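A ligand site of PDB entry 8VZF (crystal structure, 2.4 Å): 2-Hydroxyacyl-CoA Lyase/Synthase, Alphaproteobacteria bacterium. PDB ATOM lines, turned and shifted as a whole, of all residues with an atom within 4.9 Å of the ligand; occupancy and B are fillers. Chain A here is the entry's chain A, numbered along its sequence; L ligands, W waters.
A nitrogen (N4) of the ligand lies within hydrogen-bond range of the backbone NH of Gly 324 (2.8 Å).
OD2 of Asp 304 sits at hydrogen-bond distance from O9 of the ligand, 2.8 Å away.
The side-chain carboxylate (OD1) of Asp 323 is in hydrogen-bond range of a nitrogen (N3) of the ligand (2.7 Å).
An oxygen (O5) of the ligand is in salt-bridge range of the guanidinium group of Arg 281 (3.1 Å).
O5 of the ligand lies close to N of Arg 281, at 3.4 Å.
An oxygen (O2) of the ligand is in hydrogen-bond range of the side-chain hydroxyl (OG1) of Thr 246 (2.6 Å).
NH2 of Arg 161 is in hydrogen-bond range of O9 of the ligand (2.7 Å).
The backbone NH (N) of Leu 305 sits at hydrogen-bond distance from a nitrogen (N5) of the ligand (3.3 Å).
The backbone NH of Lys 221 is in hydrogen-bond range of an oxygen (O2) of the ligand (3.1 Å).
The side-chain amino group (NZ) of Lys 221 is in salt-bridge range of an oxygen (O4) of the ligand (2.5 Å).
The backbone carbonyl oxygen (O) of Arg 281 sits close to the side-chain amide oxygen (OD1) of Asn 283 (3.4 Å).
The side-chain hydroxyl (OG) of Ser 226 lies within hydrogen-bond range of the side-chain carboxylate (OD1) of Asp 323 (2.8 Å).
The side-chain amino group (NZ) of Lys 221 lies within hydrogen-bond range of the side-chain hydroxyl (OG) of Ser 421 (3.0 Å).
The backbone carbonyl oxygen (O) of Asp 304 lies within hydrogen-bond range of the backbone NH (N) of Gly 322 (3.0 Å).
N of Ser 306 lies within hydrogen-bond range of OD1 of Asp 304.
O of Gly 279 lies within hydrogen-bond range of N of Gly 222.
The backbone NH (N) of Leu 305 lies close to the backbone carbonyl oxygen (O) of Gly 322 (3.4 Å).
The backbone NH of Ile 285 lies close to the side-chain amide oxygen of Asn 283.
Water W1 lies within hydrogen-bond range of an oxygen (O5) of the ligand, the side-chain hydroxyl of Ser 421 and the side-chain amide nitrogen of Asn 283.
Water W2 bridges a nitrogen (N3) of the ligand (3.2 Å) and the indole nitrogen of Trp 225 (3.3 Å).
An oxygen (O7) of the ligand lies close to the backbone carbonyl oxygen (O) of Gly 279 (3.4 Å).
Cys 101 touches the ligand.
Gly 220 touches the ligand.
Gly 222 touches the ligand.
Trp 225 touches the ligand.
Ser 226 touches the ligand.
CA of Ala 280 touches O7 of the ligand, at 3.8 Å.
Ile 285 touches the ligand (CD1 to O1, 3.6 Å).
Ser 306 touches the ligand (CB to O10, 3.9 Å).
Gly 322 touches the ligand (O to C9, 3.6 Å).
OG of Ser 421 touches O4 of the ligand, at 3.7 Å.
19 residues have an atom within 4 Å of the ligand: Cys 101, Arg 161, Gly 220, Lys 221, Gly 222, Trp 225, Ser 226, Thr 246, Gly 279, Ala 280, Arg 281, Ile 285, Asp 304, Leu 305, Ser 306, Gly 322, Asp 323, Gly 324 and Ser 421.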
ATOM      1  N   ASN A 100      29.315  27.702  20.751  1.00  0.00           N
ATOM      2  CA  ASN A 100      29.530  26.678  19.744  1.00  0.00           C
ATOM      3  C   ASN A 100      28.323  26.451  18.843  1.00  0.00           C
ATOM      4  O   ASN A 100      28.387  25.597  17.953  1.00  0.00           O
ATOM      5  CB  ASN A 100      29.914  25.353  20.401  1.00  0.00           C
ATOM      6  CG  ASN A 100      31.281  25.393  21.038  1.00  0.00           C
ATOM      7  OD1 ASN A 100      32.299  25.259  20.358  1.00  0.00           O
ATOM      8  ND2 ASN A 100      31.316  25.575  22.353  1.00  0.00           N
ATOM      9  N   CYS A 101      27.232  27.198  19.037  1.00  0.00           N
ATOM     10  CA  CYS A 101      25.991  27.012  18.285  1.00  0.00           C
ATOM     11  C   CYS A 101      25.497  25.566  18.390  1.00  0.00           C
ATOM     12  O   CYS A 101      25.145  24.931  17.404  1.00  0.00           O
ATOM     13  CB  CYS A 101      26.161  27.426  16.826  1.00  0.00           C
ATOM     14  SG  CYS A 101      26.736  29.120  16.592  1.00  0.00           S
ATOM     15  N   ARG A 161      19.907  28.692  13.841  1.00  0.00           N
ATOM     16  CA  ARG A 161      21.217  28.551  14.466  1.00  0.00           C
ATOM     17  C   ARG A 161      21.036  27.939  15.848  1.00  0.00           C
ATOM     18  O   ARG A 161      20.412  28.569  16.718  1.00  0.00           O
ATOM     19  CB  ARG A 161      21.917  29.898  14.569  1.00  0.00           C
ATOM     20  CG  ARG A 161      23.275  29.830  15.283  1.00  0.00           C
ATOM     21  CD  ARG A 161      23.944  31.195  15.358  1.00  0.00           C
ATOM     22  NE  ARG A 161      25.107  31.281  14.475  1.00  0.00           N
ATOM     23  CZ  ARG A 161      25.913  32.333  14.399  1.00  0.00           C
ATOM     24  NH1 ARG A 161      25.720  33.401  15.152  1.00  0.00           N
ATOM     25  NH2 ARG A 161      26.940  32.300  13.555  1.00  0.00           N
ATOM     26  N   PRO A 162      21.544  26.729  16.101  1.00  0.00           N
ATOM     27  CA  PRO A 162      21.240  26.055  17.362  1.00  0.00           C
ATOM     28  C   PRO A 162      21.811  26.789  18.566  1.00  0.00           C
ATOM     29  O   PRO A 162      22.782  27.541  18.480  1.00  0.00           O
ATOM     30  CB  PRO A 162      21.906  24.674  17.190  1.00  0.00           C
ATOM     31  CG  PRO A 162      22.107  24.526  15.709  1.00  0.00           C
ATOM     32  CD  PRO A 162      22.365  25.901  15.201  1.00  0.00           C
ATOM     33  N   GLY A 220      34.198  23.529   8.272  1.00  0.00           N
ATOM     34  CA  GLY A 220      33.929  23.773   9.674  1.00  0.00           C
ATOM     35  C   GLY A 220      32.966  22.758  10.276  1.00  0.00           C
ATOM     36  O   GLY A 220      32.366  21.943   9.573  1.00  0.00           O
ATOM     37  N   LYS A 221      32.826  22.833  11.604  1.00  0.00           N
ATOM     38  CA  LYS A 221      31.967  21.880  12.302  1.00  0.00           C
ATOM     39  C   LYS A 221      30.486  22.167  12.091  1.00  0.00           C
ATOM     40  O   LYS A 221      29.650  21.326  12.469  1.00  0.00           O
ATOM     41  CB  LYS A 221      32.292  21.861  13.798  1.00  0.00           C
ATOM     42  CG  LYS A 221      31.899  23.107  14.569  1.00  0.00           C
ATOM     43  CD  LYS A 221      32.101  22.884  16.067  1.00  0.00           C
ATOM     44  CE  LYS A 221      31.618  24.070  16.899  1.00  0.00           C
ATOM     45  NZ  LYS A 221      32.473  25.278  16.725  1.00  0.00           N
ATOM     46  N   GLY A 222      30.132  23.319  11.519  1.00  0.00           N
ATOM     47  CA  GLY A 222      28.746  23.546  11.132  1.00  0.00           C
ATOM     48  C   GLY A 222      28.278  22.576  10.061  1.00  0.00           C
ATOM     49  O   GLY A 222      27.089  22.283   9.970  1.00  0.00           O
ATOM     50  N   TRP A 225      27.466  19.291  11.982  1.00  0.00           N
ATOM     51  CA  TRP A 225      26.147  19.391  12.594  1.00  0.00           C
ATOM     52  C   TRP A 225      25.040  19.205  11.561  1.00  0.00           C
ATOM     53  O   TRP A 225      24.040  18.530  11.831  1.00  0.00           O
ATOM     54  CB  TRP A 225      25.980  20.734  13.309  1.00  0.00           C
ATOM     55  CG  TRP A 225      24.557  21.032  13.652  1.00  0.00           C
ATOM     56  CD1 TRP A 225      23.748  21.961  13.060  1.00  0.00           C
ATOM     57  CD2 TRP A 225      23.764  20.369  14.645  1.00  0.00           C
ATOM     58  NE1 TRP A 225      22.500  21.933  13.637  1.00  0.00           N
ATOM     59  CE2 TRP A 225      22.489  20.968  14.611  1.00  0.00           C
ATOM     60  CE3 TRP A 225      24.015  19.348  15.559  1.00  0.00           C
ATOM     61  CZ2 TRP A 225      21.459  20.563  15.462  1.00  0.00           C
ATOM     62  CZ3 TRP A 225      22.990  18.956  16.411  1.00  0.00           C
ATOM     63  CH2 TRP A 225      21.728  19.558  16.349  1.00  0.00           C
ATOM     64  N   SER A 226      25.208  19.783  10.374  1.00  0.00           N
ATOM     65  CA  SER A 226      24.243  19.663   9.303  1.00  0.00           C
ATOM     66  C   SER A 226      24.167  18.259   8.722  1.00  0.00           C
ATOM     67  O   SER A 226      23.309  18.006   7.861  1.00  0.00           O
ATOM     68  CB  SER A 226      24.562  20.675   8.189  1.00  0.00           C
ATOM     69  OG  SER A 226      23.622  20.606   7.136  1.00  0.00           O
ATOM     70  N   THR A 246      38.782  22.344  10.195  1.00  0.00           N
ATOM     71  CA  THR A 246      38.863  23.039  11.472  1.00  0.00           C
ATOM     72  C   THR A 246      39.021  22.004  12.585  1.00  0.00           C
ATOM     73  O   THR A 246      38.918  20.802  12.335  1.00  0.00           O
ATOM     74  CB  THR A 246      37.632  23.914  11.674  1.00  0.00           C
ATOM     75  OG1 THR A 246      36.452  23.097  11.737  1.00  0.00           O
ATOM     76  CG2 THR A 246      37.482  24.924  10.544  1.00  0.00           C
ATOM     77  N   GLY A 249      35.861  20.253  12.868  1.00  0.00           N
ATOM     78  CA  GLY A 249      35.483  19.880  11.525  1.00  0.00           C
ATOM     79  C   GLY A 249      36.228  18.681  10.998  1.00  0.00           C
ATOM     80  O   GLY A 249      35.816  18.095   9.988  1.00  0.00           O
ATOM     81  N   GLY A 279      30.483  26.266   6.619  1.00  0.00           N
ATOM     82  CA  GLY A 279      30.067  26.186   8.005  1.00  0.00           C
ATOM     83  C   GLY A 279      31.163  26.517   8.997  1.00  0.00           C
ATOM     84  O   GLY A 279      31.292  25.848  10.029  1.00  0.00           O
ATOM     85  N   ALA A 280      31.968  27.540   8.689  1.00  0.00           N
ATOM     86  CA  ALA A 280      33.076  27.956   9.535  1.00  0.00           C
ATOM     87  C   ALA A 280      33.057  29.473   9.659  1.00  0.00           C
ATOM     88  O   ALA A 280      32.771  30.186   8.696  1.00  0.00           O
ATOM     89  CB  ALA A 280      34.425  27.489   8.971  1.00  0.00           C
ATOM     90  N   ARG A 281      33.382  29.962  10.854  1.00  0.00           N
ATOM     91  CA  ARG A 281      33.371  31.387  11.136  1.00  0.00           C
ATOM     92  C   ARG A 281      34.775  31.967  11.026  1.00  0.00           C
ATOM     93  O   ARG A 281      35.783  31.284  11.267  1.00  0.00           O
ATOM     94  CB  ARG A 281      32.820  31.665  12.537  1.00  0.00           C
ATOM     95  CG  ARG A 281      31.302  31.592  12.652  1.00  0.00           C
ATOM     96  CD  ARG A 281      30.829  31.889  14.068  1.00  0.00           C
ATOM     97  NE  ARG A 281      31.165  30.810  14.995  1.00  0.00           N
ATOM     98  CZ  ARG A 281      30.733  30.743  16.247  1.00  0.00           C
ATOM     99  NH1 ARG A 281      29.962  31.690  16.773  1.00  0.00           N
ATOM    100  NH2 ARG A 281      31.072  29.700  16.992  1.00  0.00           N
ATOM    101  N   ASN A 283      36.304  33.777  13.052  1.00  0.00           N
ATOM    102  CA  ASN A 283      36.588  34.182  14.415  1.00  0.00           C
ATOM    103  C   ASN A 283      38.046  33.835  14.747  1.00  0.00           C
ATOM    104  O   ASN A 283      38.880  33.664  13.843  1.00  0.00           O
ATOM    105  CB  ASN A 283      35.580  33.523  15.376  1.00  0.00           C
ATOM    106  CG  ASN A 283      35.750  32.023  15.487  1.00  0.00           C
ATOM    107  OD1 ASN A 283      36.370  31.387  14.630  1.00  0.00           O
ATOM    108  ND2 ASN A 283      35.207  31.442  16.542  1.00  0.00           N
ATOM    109  N   ILE A 285      39.459  31.195  15.757  1.00  0.00           N
ATOM    110  CA  ILE A 285      39.940  29.882  15.322  1.00  0.00           C
ATOM    111  C   ILE A 285      40.528  29.964  13.921  1.00  0.00           C
ATOM    112  O   ILE A 285      41.594  29.404  13.643  1.00  0.00           O
ATOM    113  CB  ILE A 285      38.814  28.838  15.420  1.00  0.00           C
ATOM    114  CG1 ILE A 285      38.647  28.372  16.870  1.00  0.00           C
ATOM    115  CG2 ILE A 285      39.091  27.653  14.508  1.00  0.00           C
ATOM    116  CD1 ILE A 285      37.656  27.239  17.044  1.00  0.00           C
ATOM    117  N   LEU A 286      39.860  30.691  13.016  1.00  0.00           N
ATOM    118  CA  LEU A 286      40.364  30.890  11.665  1.00  0.00           C
ATOM    119  C   LEU A 286      41.102  32.218  11.523  1.00  0.00           C
ATOM    120  O   LEU A 286      41.273  32.698  10.398  1.00  0.00           O
ATOM    121  CB  LEU A 286      39.225  30.797  10.657  1.00  0.00           C
ATOM    122  CG  LEU A 286      38.736  29.365  10.402  1.00  0.00           C
ATOM    123  CD1 LEU A 286      37.634  29.357   9.358  1.00  0.00           C
ATOM    124  CD2 LEU A 286      39.898  28.484   9.977  1.00  0.00           C
ATOM    125  N   LEU A 303      29.566  29.942   3.264  1.00  0.00           N
ATOM    126  CA  LEU A 303      28.355  29.150   3.420  1.00  0.00           C
ATOM    127  C   LEU A 303      28.046  29.073   4.915  1.00  0.00           C
ATOM    128  O   LEU A 303      28.736  28.361   5.660  1.00  0.00           O
ATOM    129  CB  LEU A 303      28.530  27.760   2.826  1.00  0.00           C
ATOM    130  CG  LEU A 303      27.298  26.908   2.493  1.00  0.00           C
ATOM    131  CD1 LEU A 303      27.713  25.692   1.695  1.00  0.00           C
ATOM    132  CD2 LEU A 303      26.535  26.474   3.744  1.00  0.00           C
ATOM    133  N   ASP A 304      27.015  29.785   5.340  1.00  0.00           N
ATOM    134  CA  ASP A 304      26.608  29.762   6.741  1.00  0.00           C
ATOM    135  C   ASP A 304      25.090  29.794   6.816  1.00  0.00           C
ATOM    136  O   ASP A 304      24.408  30.287   5.907  1.00  0.00           O
ATOM    137  CB  ASP A 304      27.215  30.947   7.513  1.00  0.00           C
ATOM    138  CG  ASP A 304      27.175  30.736   9.022  1.00  0.00           C
ATOM    139  OD1 ASP A 304      26.068  30.594   9.582  1.00  0.00           O
ATOM    140  OD2 ASP A 304      28.259  30.720   9.647  1.00  0.00           O
ATOM    141  N   LEU A 305      24.550  29.249   7.907  1.00  0.00           N
ATOM    142  CA  LEU A 305      23.112  29.291   8.135  1.00  0.00           C
ATOM    143  C   LEU A 305      22.667  30.666   8.640  1.00  0.00           C
ATOM    144  O   LEU A 305      21.580  31.129   8.294  1.00  0.00           O
ATOM    145  CB  LEU A 305      22.697  28.199   9.113  1.00  0.00           C
ATOM    146  CG  LEU A 305      21.226  28.155   9.528  1.00  0.00           C
ATOM    147  CD1 LEU A 305      20.330  27.982   8.324  1.00  0.00           C
ATOM    148  CD2 LEU A 305      21.002  27.037  10.535  1.00  0.00           C
ATOM    149  N   SER A 306      23.496  31.323   9.447  1.00  0.00           N
ATOM    150  CA  SER A 306      23.180  32.648   9.970  1.00  0.00           C
ATOM    151  C   SER A 306      23.535  33.700   8.924  1.00  0.00           C
ATOM    152  O   SER A 306      24.689  33.834   8.529  1.00  0.00           O
ATOM    153  CB  SER A 306      23.936  32.897  11.274  1.00  0.00           C
ATOM    154  OG  SER A 306      23.631  34.181  11.797  1.00  0.00           O
ATOM    155  N   GLU A 309      26.055  36.406  10.082  1.00  0.00           N
ATOM    156  CA  GLU A 309      27.469  36.043  10.146  1.00  0.00           C
ATOM    157  C   GLU A 309      28.203  36.353   8.847  1.00  0.00           C
ATOM    158  O   GLU A 309      29.431  36.440   8.851  1.00  0.00           O
ATOM    159  CB  GLU A 309      27.603  34.555  10.491  1.00  0.00           C
ATOM    160  CG  GLU A 309      29.019  34.088  10.779  1.00  0.00           C
ATOM    161  CD  GLU A 309      29.584  34.668  12.063  1.00  0.00           C
ATOM    162  OE1 GLU A 309      28.853  34.693  13.069  1.00  0.00           O
ATOM    163  OE2 GLU A 309      30.755  35.108  12.061  1.00  0.00           O
ATOM    164  N   GLY A 322      22.130  29.564   4.102  1.00  0.00           N
ATOM    165  CA  GLY A 322      21.236  28.430   4.170  1.00  0.00           C
ATOM    166  C   GLY A 322      21.913  27.261   4.859  1.00  0.00           C
ATOM    167  O   GLY A 322      22.918  27.428   5.552  1.00  0.00           O
ATOM    168  N   ASP A 323      21.347  26.077   4.647  1.00  0.00           N
ATOM    169  CA  ASP A 323      21.853  24.853   5.268  1.00  0.00           C
ATOM    170  C   ASP A 323      23.036  24.299   4.487  1.00  0.00           C
ATOM    171  O   ASP A 323      23.066  24.350   3.254  1.00  0.00           O
ATOM    172  CB  ASP A 323      20.748  23.810   5.358  1.00  0.00           C
ATOM    173  CG  ASP A 323      21.217  22.509   5.951  1.00  0.00           C
ATOM    174  OD1 ASP A 323      21.474  22.475   7.179  1.00  0.00           O
ATOM    175  OD2 ASP A 323      21.345  21.513   5.200  1.00  0.00           O
ATOM    176  N   GLY A 324      24.005  23.741   5.217  1.00  0.00           N
ATOM    177  CA  GLY A 324      25.194  23.193   4.608  1.00  0.00           C
ATOM    178  C   GLY A 324      24.942  22.048   3.643  1.00  0.00           C
ATOM    179  O   GLY A 324      25.342  22.118   2.480  1.00  0.00           O
ATOM    180  N   SER A 421      34.903  26.522  20.561  1.00  0.00           N
ATOM    181  CA  SER A 421      35.024  27.942  20.257  1.00  0.00           C
ATOM    182  C   SER A 421      35.156  28.806  21.504  1.00  0.00           C
ATOM    183  O   SER A 421      35.505  29.987  21.379  1.00  0.00           O
ATOM    184  CB  SER A 421      33.819  28.399  19.436  1.00  0.00           C
ATOM    185  OG  SER A 421      33.674  27.621  18.260  1.00  0.00           O
HETATM  186  P1  LIG L   1      34.687  26.038  13.562  1.00  0.00           P
HETATM  187  O1  LIG L   1      34.879  26.235  15.054  1.00  0.00           O
HETATM  188  O2  LIG L   1      34.917  24.622  13.095  1.00  0.00           O
HETATM  189  O3  LIG L   1      35.330  27.092  12.704  1.00  0.00           O
HETATM  190  P2  LIG L   1      32.327  27.508  13.985  1.00  0.00           P
HETATM  191  O4  LIG L   1      31.640  27.049  15.245  1.00  0.00           O
HETATM  192  O5  LIG L   1      33.235  28.720  14.019  1.00  0.00           O
HETATM  193  O6  LIG L   1      33.111  26.252  13.337  1.00  0.00           O
HETATM  194  O7  LIG L   1      31.197  27.762  12.867  1.00  0.00           O
HETATM  195  C1  LIG L   1      29.865  27.323  13.108  1.00  0.00           C
HETATM  196  C2  LIG L   1      28.929  28.019  12.134  1.00  0.00           C
HETATM  197  O8  LIG L   1      28.109  27.076  11.448  1.00  0.00           O
HETATM  198  C3  LIG L   1      27.991  28.968  12.880  1.00  0.00           C
HETATM  199  O9  LIG L   1      28.194  30.286  12.365  1.00  0.00           O
HETATM  200  C4  LIG L   1      26.589  28.485  12.545  1.00  0.00           C
HETATM  201  O10 LIG L   1      25.731  29.594  12.290  1.00  0.00           O
HETATM  202  C5  LIG L   1      26.800  27.634  11.313  1.00  0.00           C
HETATM  203  N1  LIG L   1      25.773  26.566  11.162  1.00  0.00           N
HETATM  204  C6  LIG L   1      25.089  25.957  12.140  1.00  0.00           C
HETATM  205  N2  LIG L   1      24.217  25.038  11.630  1.00  0.00           N
HETATM  206  C7  LIG L   1      24.344  25.064  10.289  1.00  0.00           C
HETATM  207  C8  LIG L   1      23.739  24.356   9.134  1.00  0.00           C
HETATM  208  N3  LIG L   1      22.789  23.403   9.304  1.00  0.00           N
HETATM  209  N4  LIG L   1      24.168  24.691   7.897  1.00  0.00           N
HETATM  210  C9  LIG L   1      25.106  25.633   7.709  1.00  0.00           C
HETATM  211  N5  LIG L   1      25.709  26.312   8.697  1.00  0.00           N
HETATM  212  C10 LIG L   1      25.370  26.081   9.988  1.00  0.00           C
HETATM  213  O   HOH W   1      34.777  28.702  16.099  1.00  0.00           O
HETATM  214  O   HOH W   2      20.336  22.603  11.243  1.00  0.00           O
